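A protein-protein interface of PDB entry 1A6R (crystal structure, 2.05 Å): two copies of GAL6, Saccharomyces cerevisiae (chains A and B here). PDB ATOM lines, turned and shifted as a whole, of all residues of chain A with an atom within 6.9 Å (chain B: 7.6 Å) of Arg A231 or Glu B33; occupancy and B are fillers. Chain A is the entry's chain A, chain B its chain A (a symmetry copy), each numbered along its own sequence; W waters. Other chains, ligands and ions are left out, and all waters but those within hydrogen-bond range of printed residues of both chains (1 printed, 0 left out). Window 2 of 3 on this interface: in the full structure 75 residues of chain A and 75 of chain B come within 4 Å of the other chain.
The side-chain carboxylate (OE2) of Glu A227 is in salt-bridge range of the side-chain amino group (NZ) of Lys B26 (2.9 Å). NH2 of Arg A231 is in salt-bridge range of OE2 of Glu B33 (2.6 Å).
The guanidinium group of Arg A235 is in salt-bridge range of the side-chain carboxylate of Glu A232 (2.8 Å). The side-chain hydroxyl of Ser B36 is in hydrogen-bond range of the backbone carbonyl oxygen of Glu B33 (2.9 Å). OD2 of Asp B37 lies within hydrogen-bond range of N of His B40 (3.0 Å).
CG of Gln A230 touches CD1 of Ile B22, 3.8 Å away. Gln A230 touches Trp B30 (OE1 to CH2, 3.5 Å). Arg A231 touches Trp B30 (NE to NE1, 3.6 Å). Arg A231 touches Phe B34. Phe A234 touches Ile B27. N of Asn B31 touches CE2 of Phe A234 (3.8 Å). CE2 of Phe B34 touches CD2 of Phe A234, at 3.9 Å. Arg A235 touches Phe B34. His B40 touches Arg A235 (CE1 to O, 3.8 Å).
No position is printed for both chains. Of the 11 pairs that touch across the chains among the printed residues, none has its exchanged pair printed and touching as well.
Water W1 lies within hydrogen-bond range of the side-chain amino group of Lys B26 (2.5 Å) and the side-chain amide oxygen of Gln A230 (2.6 Å).
Of the 15 printed residues of chain B, 8 touch a printed residue of chain A. Printed residues of chain B that touch a printed residue of chain A: Ile B22, Lys B26, Ile B27, Trp B30, Asn B31, Glu B33, Phe B34 and His B40. Along chain B the printed residues that touch a printed residue of chain A span positions 22 to 40. Hydrophobic or aromatic side chains of chain A within 4 Å of the printed part of chain B: Phe A234.
Arg A231 touches three residues of chain B. Printed residues of chain B within 4 Å of Arg A235: Phe B34 and His B40. Printed residues of chain B within 4 Å of Gln A230: Ile B22 and Trp B30. The nearest residue of chain B that does not touch Arg A231 is Lys B26 (6.8 Å). The nearest printed residue of chain A that does not touch Glu B33 is Phe A234 (7.7 Å). The nearest printed residue of chain A that does not touch His B40 is Leu A236 (5.9 Å).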
ATOM      1  N   ARG A 226      -9.103   5.196  -4.346  1.00  0.00           N
ATOM      2  CA  ARG A 226      -9.384   3.775  -4.356  1.00  0.00           C
ATOM      3  C   ARG A 226      -8.730   3.057  -5.540  1.00  0.00           C
ATOM      4  O   ARG A 226      -8.143   1.980  -5.380  1.00  0.00           O
ATOM      5  CB  ARG A 226     -10.900   3.512  -4.339  1.00  0.00           C
ATOM      6  CG  ARG A 226     -11.533   3.750  -2.999  1.00  0.00           C
ATOM      7  CD  ARG A 226     -13.035   3.609  -3.094  1.00  0.00           C
ATOM      8  NE  ARG A 226     -13.488   2.226  -3.183  1.00  0.00           N
ATOM      9  CZ  ARG A 226     -14.694   1.826  -2.802  1.00  0.00           C
ATOM     10  NH1 ARG A 226     -15.544   2.714  -2.311  1.00  0.00           N
ATOM     11  NH2 ARG A 226     -15.068   0.557  -2.931  1.00  0.00           N
ATOM     12  N   GLU A 227      -8.849   3.634  -6.729  1.00  0.00           N
ATOM     13  CA  GLU A 227      -8.270   3.006  -7.893  1.00  0.00           C
ATOM     14  C   GLU A 227      -6.762   2.845  -7.753  1.00  0.00           C
ATOM     15  O   GLU A 227      -6.213   1.794  -8.082  1.00  0.00           O
ATOM     16  CB  GLU A 227      -8.618   3.755  -9.162  1.00  0.00           C
ATOM     17  CG  GLU A 227      -8.499   2.850 -10.392  1.00  0.00           C
ATOM     18  CD  GLU A 227      -8.438   3.639 -11.673  1.00  0.00           C
ATOM     19  OE1 GLU A 227      -8.139   4.858 -11.591  1.00  0.00           O
ATOM     20  OE2 GLU A 227      -8.685   3.050 -12.753  1.00  0.00           O
ATOM     21  N   GLN A 228      -6.091   3.858  -7.235  1.00  0.00           N
ATOM     22  CA  GLN A 228      -4.653   3.748  -7.042  1.00  0.00           C
ATOM     23  C   GLN A 228      -4.365   2.611  -6.053  1.00  0.00           C
ATOM     24  O   GLN A 228      -3.379   1.881  -6.199  1.00  0.00           O
ATOM     25  CB  GLN A 228      -4.082   5.049  -6.493  1.00  0.00           C
ATOM     26  CG  GLN A 228      -4.282   6.232  -7.404  1.00  0.00           C
ATOM     27  CD  GLN A 228      -4.045   7.559  -6.702  1.00  0.00           C
ATOM     28  OE1 GLN A 228      -3.738   7.612  -5.507  1.00  0.00           O
ATOM     29  NE2 GLN A 228      -4.186   8.645  -7.450  1.00  0.00           N
ATOM     30  N   MET A 229      -5.215   2.488  -5.035  1.00  0.00           N
ATOM     31  CA  MET A 229      -5.057   1.447  -4.031  1.00  0.00           C
ATOM     32  C   MET A 229      -5.210   0.091  -4.680  1.00  0.00           C
ATOM     33  O   MET A 229      -4.407  -0.807  -4.470  1.00  0.00           O
ATOM     34  CB  MET A 229      -6.072   1.647  -2.909  1.00  0.00           C
ATOM     35  CG  MET A 229      -5.634   2.726  -1.965  1.00  0.00           C
ATOM     36  SD  MET A 229      -6.821   3.074  -0.680  1.00  0.00           S
ATOM     37  CE  MET A 229      -5.848   4.141   0.206  1.00  0.00           C
ATOM     38  N   GLN A 230      -6.205  -0.020  -5.540  1.00  0.00           N
ATOM     39  CA  GLN A 230      -6.474  -1.248  -6.264  1.00  0.00           C
ATOM     40  C   GLN A 230      -5.287  -1.618  -7.189  1.00  0.00           C
ATOM     41  O   GLN A 230      -4.931  -2.790  -7.342  1.00  0.00           O
ATOM     42  CB  GLN A 230      -7.743  -1.047  -7.075  1.00  0.00           C
ATOM     43  CG  GLN A 230      -8.567  -2.256  -7.255  1.00  0.00           C
ATOM     44  CD  GLN A 230      -9.669  -2.029  -8.243  1.00  0.00           C
ATOM     45  OE1 GLN A 230      -9.414  -1.703  -9.404  1.00  0.00           O
ATOM     46  NE2 GLN A 230     -10.910  -2.170  -7.796  1.00  0.00           N
ATOM     47  N   ARG A 231      -4.672  -0.611  -7.801  1.00  0.00           N
ATOM     48  CA  ARG A 231      -3.543  -0.838  -8.702  1.00  0.00           C
ATOM     49  C   ARG A 231      -2.313  -1.320  -7.932  1.00  0.00           C
ATOM     50  O   ARG A 231      -1.563  -2.191  -8.397  1.00  0.00           O
ATOM     51  CB  ARG A 231      -3.224   0.468  -9.423  1.00  0.00           C
ATOM     52  CG  ARG A 231      -2.047   0.427 -10.369  1.00  0.00           C
ATOM     53  CD  ARG A 231      -1.843   1.814 -10.952  1.00  0.00           C
ATOM     54  NE  ARG A 231      -1.069   1.761 -12.183  1.00  0.00           N
ATOM     55  CZ  ARG A 231       0.231   1.991 -12.243  1.00  0.00           C
ATOM     56  NH1 ARG A 231       0.908   2.290 -11.145  1.00  0.00           N
ATOM     57  NH2 ARG A 231       0.855   1.927 -13.394  1.00  0.00           N
ATOM     58  N   GLU A 232      -2.070  -0.697  -6.786  1.00  0.00           N
ATOM     59  CA  GLU A 232      -0.948  -1.049  -5.949  1.00  0.00           C
ATOM     60  C   GLU A 232      -1.128  -2.479  -5.392  1.00  0.00           C
ATOM     61  O   GLU A 232      -0.162  -3.237  -5.265  1.00  0.00           O
ATOM     62  CB  GLU A 232      -0.823  -0.022  -4.830  1.00  0.00           C
ATOM     63  CG  GLU A 232       0.303  -0.255  -3.840  1.00  0.00           C
ATOM     64  CD  GLU A 232       1.699  -0.308  -4.460  1.00  0.00           C
ATOM     65  OE1 GLU A 232       1.902   0.120  -5.622  1.00  0.00           O
ATOM     66  OE2 GLU A 232       2.611  -0.794  -3.761  1.00  0.00           O
ATOM     67  N   ILE A 233      -2.371  -2.844  -5.093  1.00  0.00           N
ATOM     68  CA  ILE A 233      -2.666  -4.174  -4.581  1.00  0.00           C
ATOM     69  C   ILE A 233      -2.394  -5.187  -5.680  1.00  0.00           C
ATOM     70  O   ILE A 233      -1.801  -6.241  -5.419  1.00  0.00           O
ATOM     71  CB  ILE A 233      -4.137  -4.324  -4.078  1.00  0.00           C
ATOM     72  CG1 ILE A 233      -4.332  -3.565  -2.758  1.00  0.00           C
ATOM     73  CG2 ILE A 233      -4.457  -5.787  -3.848  1.00  0.00           C
ATOM     74  CD1 ILE A 233      -3.304  -3.919  -1.669  1.00  0.00           C
ATOM     75  N   PHE A 234      -2.829  -4.871  -6.900  1.00  0.00           N
ATOM     76  CA  PHE A 234      -2.602  -5.763  -8.014  1.00  0.00           C
ATOM     77  C   PHE A 234      -1.104  -5.834  -8.245  1.00  0.00           C
ATOM     78  O   PHE A 234      -0.572  -6.923  -8.461  1.00  0.00           O
ATOM     79  CB  PHE A 234      -3.312  -5.324  -9.309  1.00  0.00           C
ATOM     80  CG  PHE A 234      -2.982  -6.199 -10.476  1.00  0.00           C
ATOM     81  CD1 PHE A 234      -3.589  -7.441 -10.617  1.00  0.00           C
ATOM     82  CD2 PHE A 234      -1.933  -5.867 -11.334  1.00  0.00           C
ATOM     83  CE1 PHE A 234      -3.149  -8.343 -11.578  1.00  0.00           C
ATOM     84  CE2 PHE A 234      -1.480  -6.768 -12.301  1.00  0.00           C
ATOM     85  CZ  PHE A 234      -2.082  -8.007 -12.422  1.00  0.00           C
ATOM     86  N   ARG A 235      -0.418  -4.700  -8.111  1.00  0.00           N
ATOM     87  CA  ARG A 235       1.017  -4.684  -8.329  1.00  0.00           C
ATOM     88  C   ARG A 235       1.740  -5.648  -7.402  1.00  0.00           C
ATOM     89  O   ARG A 235       2.571  -6.453  -7.860  1.00  0.00           O
ATOM     90  CB  ARG A 235       1.598  -3.295  -8.145  1.00  0.00           C
ATOM     91  CG  ARG A 235       3.015  -3.233  -8.647  1.00  0.00           C
ATOM     92  CD  ARG A 235       3.678  -1.934  -8.313  1.00  0.00           C
ATOM     93  NE  ARG A 235       3.833  -1.742  -6.871  1.00  0.00           N
ATOM     94  CZ  ARG A 235       4.905  -2.070  -6.161  1.00  0.00           C
ATOM     95  NH1 ARG A 235       5.952  -2.640  -6.731  1.00  0.00           N
ATOM     96  NH2 ARG A 235       4.973  -1.722  -4.890  1.00  0.00           N
ATOM     97  N   LEU A 236       1.472  -5.528  -6.102  1.00  0.00           N
ATOM     98  CA  LEU A 236       2.109  -6.401  -5.118  1.00  0.00           C
ATOM     99  C   LEU A 236       1.700  -7.874  -5.313  1.00  0.00           C
ATOM    100  O   LEU A 236       2.491  -8.782  -5.101  1.00  0.00           O
ATOM    101  CB  LEU A 236       1.776  -5.928  -3.725  1.00  0.00           C
ATOM    102  CG  LEU A 236       2.328  -4.569  -3.353  1.00  0.00           C
ATOM    103  CD1 LEU A 236       1.626  -4.081  -2.092  1.00  0.00           C
ATOM    104  CD2 LEU A 236       3.811  -4.646  -3.155  1.00  0.00           C
ATOM    105  N   MET A 237       0.477  -8.129  -5.740  1.00  0.00           N
ATOM    106  CA  MET A 237       0.100  -9.509  -5.966  1.00  0.00           C
ATOM    107  C   MET A 237       0.853 -10.171  -7.095  1.00  0.00           C
ATOM    108  O   MET A 237       1.324 -11.307  -6.950  1.00  0.00           O
ATOM    109  CB  MET A 237      -1.373  -9.615  -6.211  1.00  0.00           C
ATOM    110  CG  MET A 237      -2.058  -9.574  -4.879  1.00  0.00           C
ATOM    111  SD  MET A 237      -3.669 -10.136  -4.915  1.00  0.00           S
ATOM    112  CE  MET A 237      -3.550 -11.787  -5.749  1.00  0.00           C
ATOM    113  N   ILE B  22     -13.315  -5.140  -9.413  1.00  0.00           N
ATOM    114  CA  ILE B  22     -12.047  -5.511 -10.027  1.00  0.00           C
ATOM    115  C   ILE B  22     -12.451  -5.715 -11.472  1.00  0.00           C
ATOM    116  O   ILE B  22     -13.367  -6.482 -11.761  1.00  0.00           O
ATOM    117  CB  ILE B  22     -11.490  -6.852  -9.454  1.00  0.00           C
ATOM    118  CG1 ILE B  22     -10.847  -6.628  -8.086  1.00  0.00           C
ATOM    119  CG2 ILE B  22     -10.549  -7.537 -10.444  1.00  0.00           C
ATOM    120  CD1 ILE B  22      -9.542  -5.848  -8.120  1.00  0.00           C
ATOM    121  N   LYS B  26      -8.795  -3.972 -16.901  1.00  0.00           N
ATOM    122  CA  LYS B  26      -7.943  -3.081 -16.139  1.00  0.00           C
ATOM    123  C   LYS B  26      -6.706  -3.765 -15.549  1.00  0.00           C
ATOM    124  O   LYS B  26      -5.583  -3.284 -15.730  1.00  0.00           O
ATOM    125  CB  LYS B  26      -8.737  -2.398 -15.033  1.00  0.00           C
ATOM    126  CG  LYS B  26      -7.972  -1.288 -14.373  1.00  0.00           C
ATOM    127  CD  LYS B  26      -8.724  -0.683 -13.232  1.00  0.00           C
ATOM    128  CE  LYS B  26     -10.007  -0.019 -13.677  1.00  0.00           C
ATOM    129  NZ  LYS B  26     -10.584   0.801 -12.570  1.00  0.00           N
ATOM    130  N   ILE B  27      -6.908  -4.885 -14.844  1.00  0.00           N
ATOM    131  CA  ILE B  27      -5.785  -5.584 -14.206  1.00  0.00           C
ATOM    132  C   ILE B  27      -4.823  -6.167 -15.240  1.00  0.00           C
ATOM    133  O   ILE B  27      -3.617  -6.178 -15.029  1.00  0.00           O
ATOM    134  CB  ILE B  27      -6.252  -6.662 -13.149  1.00  0.00           C
ATOM    135  CG1 ILE B  27      -7.029  -7.794 -13.831  1.00  0.00           C
ATOM    136  CG2 ILE B  27      -7.113  -5.984 -12.063  1.00  0.00           C
ATOM    137  CD1 ILE B  27      -7.404  -8.959 -12.897  1.00  0.00           C
ATOM    138  N   ASN B  28      -5.348  -6.586 -16.379  1.00  0.00           N
ATOM    139  CA  ASN B  28      -4.498  -7.122 -17.438  1.00  0.00           C
ATOM    140  C   ASN B  28      -3.711  -5.979 -18.103  1.00  0.00           C
ATOM    141  O   ASN B  28      -2.553  -6.158 -18.497  1.00  0.00           O
ATOM    142  CB  ASN B  28      -5.325  -7.916 -18.442  1.00  0.00           C
ATOM    143  CG  ASN B  28      -5.565  -9.340 -17.985  1.00  0.00           C
ATOM    144  OD1 ASN B  28      -4.694 -10.184 -18.151  1.00  0.00           O
ATOM    145  ND2 ASN B  28      -6.737  -9.615 -17.404  1.00  0.00           N
ATOM    146  N   SER B  29      -4.305  -4.784 -18.144  1.00  0.00           N
ATOM    147  CA  SER B  29      -3.623  -3.616 -18.701  1.00  0.00           C
ATOM    148  C   SER B  29      -2.525  -3.186 -17.734  1.00  0.00           C
ATOM    149  O   SER B  29      -1.403  -2.874 -18.152  1.00  0.00           O
ATOM    150  CB  SER B  29      -4.616  -2.490 -18.948  1.00  0.00           C
ATOM    151  OG  SER B  29      -5.587  -2.912 -19.897  1.00  0.00           O
ATOM    152  N   TRP B  30      -2.826  -3.215 -16.437  1.00  0.00           N
ATOM    153  CA  TRP B  30      -1.821  -2.872 -15.445  1.00  0.00           C
ATOM    154  C   TRP B  30      -0.692  -3.914 -15.527  1.00  0.00           C
ATOM    155  O   TRP B  30       0.486  -3.577 -15.408  1.00  0.00           O
ATOM    156  CB  TRP B  30      -2.405  -2.888 -14.042  1.00  0.00           C
ATOM    157  CG  TRP B  30      -3.252  -1.721 -13.695  1.00  0.00           C
ATOM    158  CD1 TRP B  30      -3.152  -0.440 -14.188  1.00  0.00           C
ATOM    159  CD2 TRP B  30      -4.316  -1.699 -12.735  1.00  0.00           C
ATOM    160  NE1 TRP B  30      -4.092   0.374 -13.586  1.00  0.00           N
ATOM    161  CE2 TRP B  30      -4.820  -0.374 -12.691  1.00  0.00           C
ATOM    162  CE3 TRP B  30      -4.895  -2.671 -11.895  1.00  0.00           C
ATOM    163  CZ2 TRP B  30      -5.878   0.005 -11.839  1.00  0.00           C
ATOM    164  CZ3 TRP B  30      -5.950  -2.297 -11.047  1.00  0.00           C
ATOM    165  CH2 TRP B  30      -6.430  -0.970 -11.028  1.00  0.00           C
ATOM    166  N   ASN B  31      -1.054  -5.180 -15.712  1.00  0.00           N
ATOM    167  CA  ASN B  31      -0.044  -6.231 -15.806  1.00  0.00           C
ATOM    168  C   ASN B  31       0.919  -5.947 -16.966  1.00  0.00           C
ATOM    169  O   ASN B  31       2.144  -6.024 -16.808  1.00  0.00           O
ATOM    170  CB  ASN B  31      -0.688  -7.604 -16.010  1.00  0.00           C
ATOM    171  CG  ASN B  31       0.314  -8.711 -15.895  1.00  0.00           C
ATOM    172  OD1 ASN B  31       0.998  -8.836 -14.870  1.00  0.00           O
ATOM    173  ND2 ASN B  31       0.483  -9.469 -16.963  1.00  0.00           N
ATOM    174  N   LYS B  32       0.359  -5.624 -18.128  1.00  0.00           N
ATOM    175  CA  LYS B  32       1.162  -5.299 -19.303  1.00  0.00           C
ATOM    176  C   LYS B  32       2.154  -4.186 -18.964  1.00  0.00           C
ATOM    177  O   LYS B  32       3.348  -4.289 -19.256  1.00  0.00           O
ATOM    178  CB  LYS B  32       0.245  -4.867 -20.432  1.00  0.00           C
ATOM    179  CG  LYS B  32       0.865  -5.021 -21.773  1.00  0.00           C
ATOM    180  CD  LYS B  32      -0.070  -4.547 -22.870  1.00  0.00           C
ATOM    181  CE  LYS B  32       0.719  -4.328 -24.172  1.00  0.00           C
ATOM    182  NZ  LYS B  32       0.026  -3.393 -25.125  1.00  0.00           N
ATOM    183  N   GLU B  33       1.677  -3.141 -18.287  1.00  0.00           N
ATOM    184  CA  GLU B  33       2.551  -2.041 -17.917  1.00  0.00           C
ATOM    185  C   GLU B  33       3.620  -2.416 -16.888  1.00  0.00           C
ATOM    186  O   GLU B  33       4.768  -1.972 -17.019  1.00  0.00           O
ATOM    187  CB  GLU B  33       1.751  -0.864 -17.405  1.00  0.00           C
ATOM    188  CG  GLU B  33       2.619   0.246 -16.863  1.00  0.00           C
ATOM    189  CD  GLU B  33       1.822   1.339 -16.172  1.00  0.00           C
ATOM    190  OE1 GLU B  33       0.583   1.375 -16.292  1.00  0.00           O
ATOM    191  OE2 GLU B  33       2.439   2.162 -15.485  1.00  0.00           O
ATOM    192  N   PHE B  34       3.269  -3.199 -15.859  1.00  0.00           N
ATOM    193  CA  PHE B  34       4.269  -3.595 -14.848  1.00  0.00           C
ATOM    194  C   PHE B  34       5.355  -4.489 -15.430  1.00  0.00           C
ATOM    195  O   PHE B  34       6.528  -4.331 -15.116  1.00  0.00           O
ATOM    196  CB  PHE B  34       3.619  -4.286 -13.653  1.00  0.00           C
ATOM    197  CG  PHE B  34       2.733  -3.384 -12.864  1.00  0.00           C
ATOM    198  CD1 PHE B  34       3.125  -2.088 -12.584  1.00  0.00           C
ATOM    199  CD2 PHE B  34       1.485  -3.811 -12.439  1.00  0.00           C
ATOM    200  CE1 PHE B  34       2.271  -1.219 -11.892  1.00  0.00           C
ATOM    201  CE2 PHE B  34       0.630  -2.967 -11.754  1.00  0.00           C
ATOM    202  CZ  PHE B  34       1.016  -1.669 -11.479  1.00  0.00           C
ATOM    203  N   GLN B  35       4.959  -5.394 -16.312  1.00  0.00           N
ATOM    204  CA  GLN B  35       5.897  -6.307 -16.941  1.00  0.00           C
ATOM    205  C   GLN B  35       6.922  -5.639 -17.857  1.00  0.00           C
ATOM    206  O   GLN B  35       7.913  -6.268 -18.226  1.00  0.00           O
ATOM    207  CB  GLN B  35       5.156  -7.403 -17.700  1.00  0.00           C
ATOM    208  CG  GLN B  35       4.386  -8.408 -16.821  1.00  0.00           C
ATOM    209  CD  GLN B  35       5.267  -9.162 -15.804  1.00  0.00           C
ATOM    210  OE1 GLN B  35       6.393  -9.572 -16.115  1.00  0.00           O
ATOM    211  NE2 GLN B  35       4.743  -9.361 -14.590  1.00  0.00           N
ATOM    212  N   SER B  36       6.688  -4.383 -18.236  1.00  0.00           N
ATOM    213  CA  SER B  36       7.631  -3.670 -19.100  1.00  0.00           C
ATOM    214  C   SER B  36       8.746  -3.072 -18.261  1.00  0.00           C
ATOM    215  O   SER B  36       9.728  -2.551 -18.778  1.00  0.00           O
ATOM    216  CB  SER B  36       6.929  -2.578 -19.925  1.00  0.00           C
ATOM    217  OG  SER B  36       6.610  -1.434 -19.139  1.00  0.00           O
ATOM    218  N   ASP B  37       8.563  -3.089 -16.951  1.00  0.00           N
ATOM    219  CA  ASP B  37       9.568  -2.552 -16.074  1.00  0.00           C
ATOM    220  C   ASP B  37      10.521  -3.691 -15.696  1.00  0.00           C
ATOM    221  O   ASP B  37      10.086  -4.746 -15.263  1.00  0.00           O
ATOM    222  CB  ASP B  37       8.908  -1.946 -14.847  1.00  0.00           C
ATOM    223  CG  ASP B  37       9.896  -1.280 -13.956  1.00  0.00           C
ATOM    224  OD1 ASP B  37      10.244  -0.109 -14.209  1.00  0.00           O
ATOM    225  OD2 ASP B  37      10.369  -1.943 -13.018  1.00  0.00           O
ATOM    226  N   LEU B  38      11.819  -3.452 -15.827  1.00  0.00           N
ATOM    227  CA  LEU B  38      12.827  -4.458 -15.543  1.00  0.00           C
ATOM    228  C   LEU B  38      12.892  -4.844 -14.066  1.00  0.00           C
ATOM    229  O   LEU B  38      13.161  -6.000 -13.731  1.00  0.00           O
ATOM    230  CB  LEU B  38      14.206  -3.974 -16.007  1.00  0.00           C
ATOM    231  CG  LEU B  38      15.207  -5.113 -16.274  1.00  0.00           C
ATOM    232  CD1 LEU B  38      14.785  -5.849 -17.556  1.00  0.00           C
ATOM    233  CD2 LEU B  38      16.636  -4.563 -16.410  1.00  0.00           C
ATOM    234  N   HIS B  40      10.426  -4.800 -12.061  1.00  0.00           N
ATOM    235  CA  HIS B  40       9.243  -5.630 -11.857  1.00  0.00           C
ATOM    236  C   HIS B  40       9.467  -7.064 -12.387  1.00  0.00           C
ATOM    237  O   HIS B  40       9.145  -8.056 -11.710  1.00  0.00           O
ATOM    238  CB  HIS B  40       7.999  -5.007 -12.521  1.00  0.00           C
ATOM    239  CG  HIS B  40       6.700  -5.636 -12.085  1.00  0.00           C
ATOM    240  ND1 HIS B  40       6.038  -5.258 -10.934  1.00  0.00           N
ATOM    241  CD2 HIS B  40       5.952  -6.617 -12.644  1.00  0.00           C
ATOM    242  CE1 HIS B  40       4.940  -5.978 -10.809  1.00  0.00           C
ATOM    243  NE2 HIS B  40       4.862  -6.812 -11.830  1.00  0.00           N
HETATM  244  O   HOH W   1     -10.719   0.439 -10.077  1.00  0.00           O
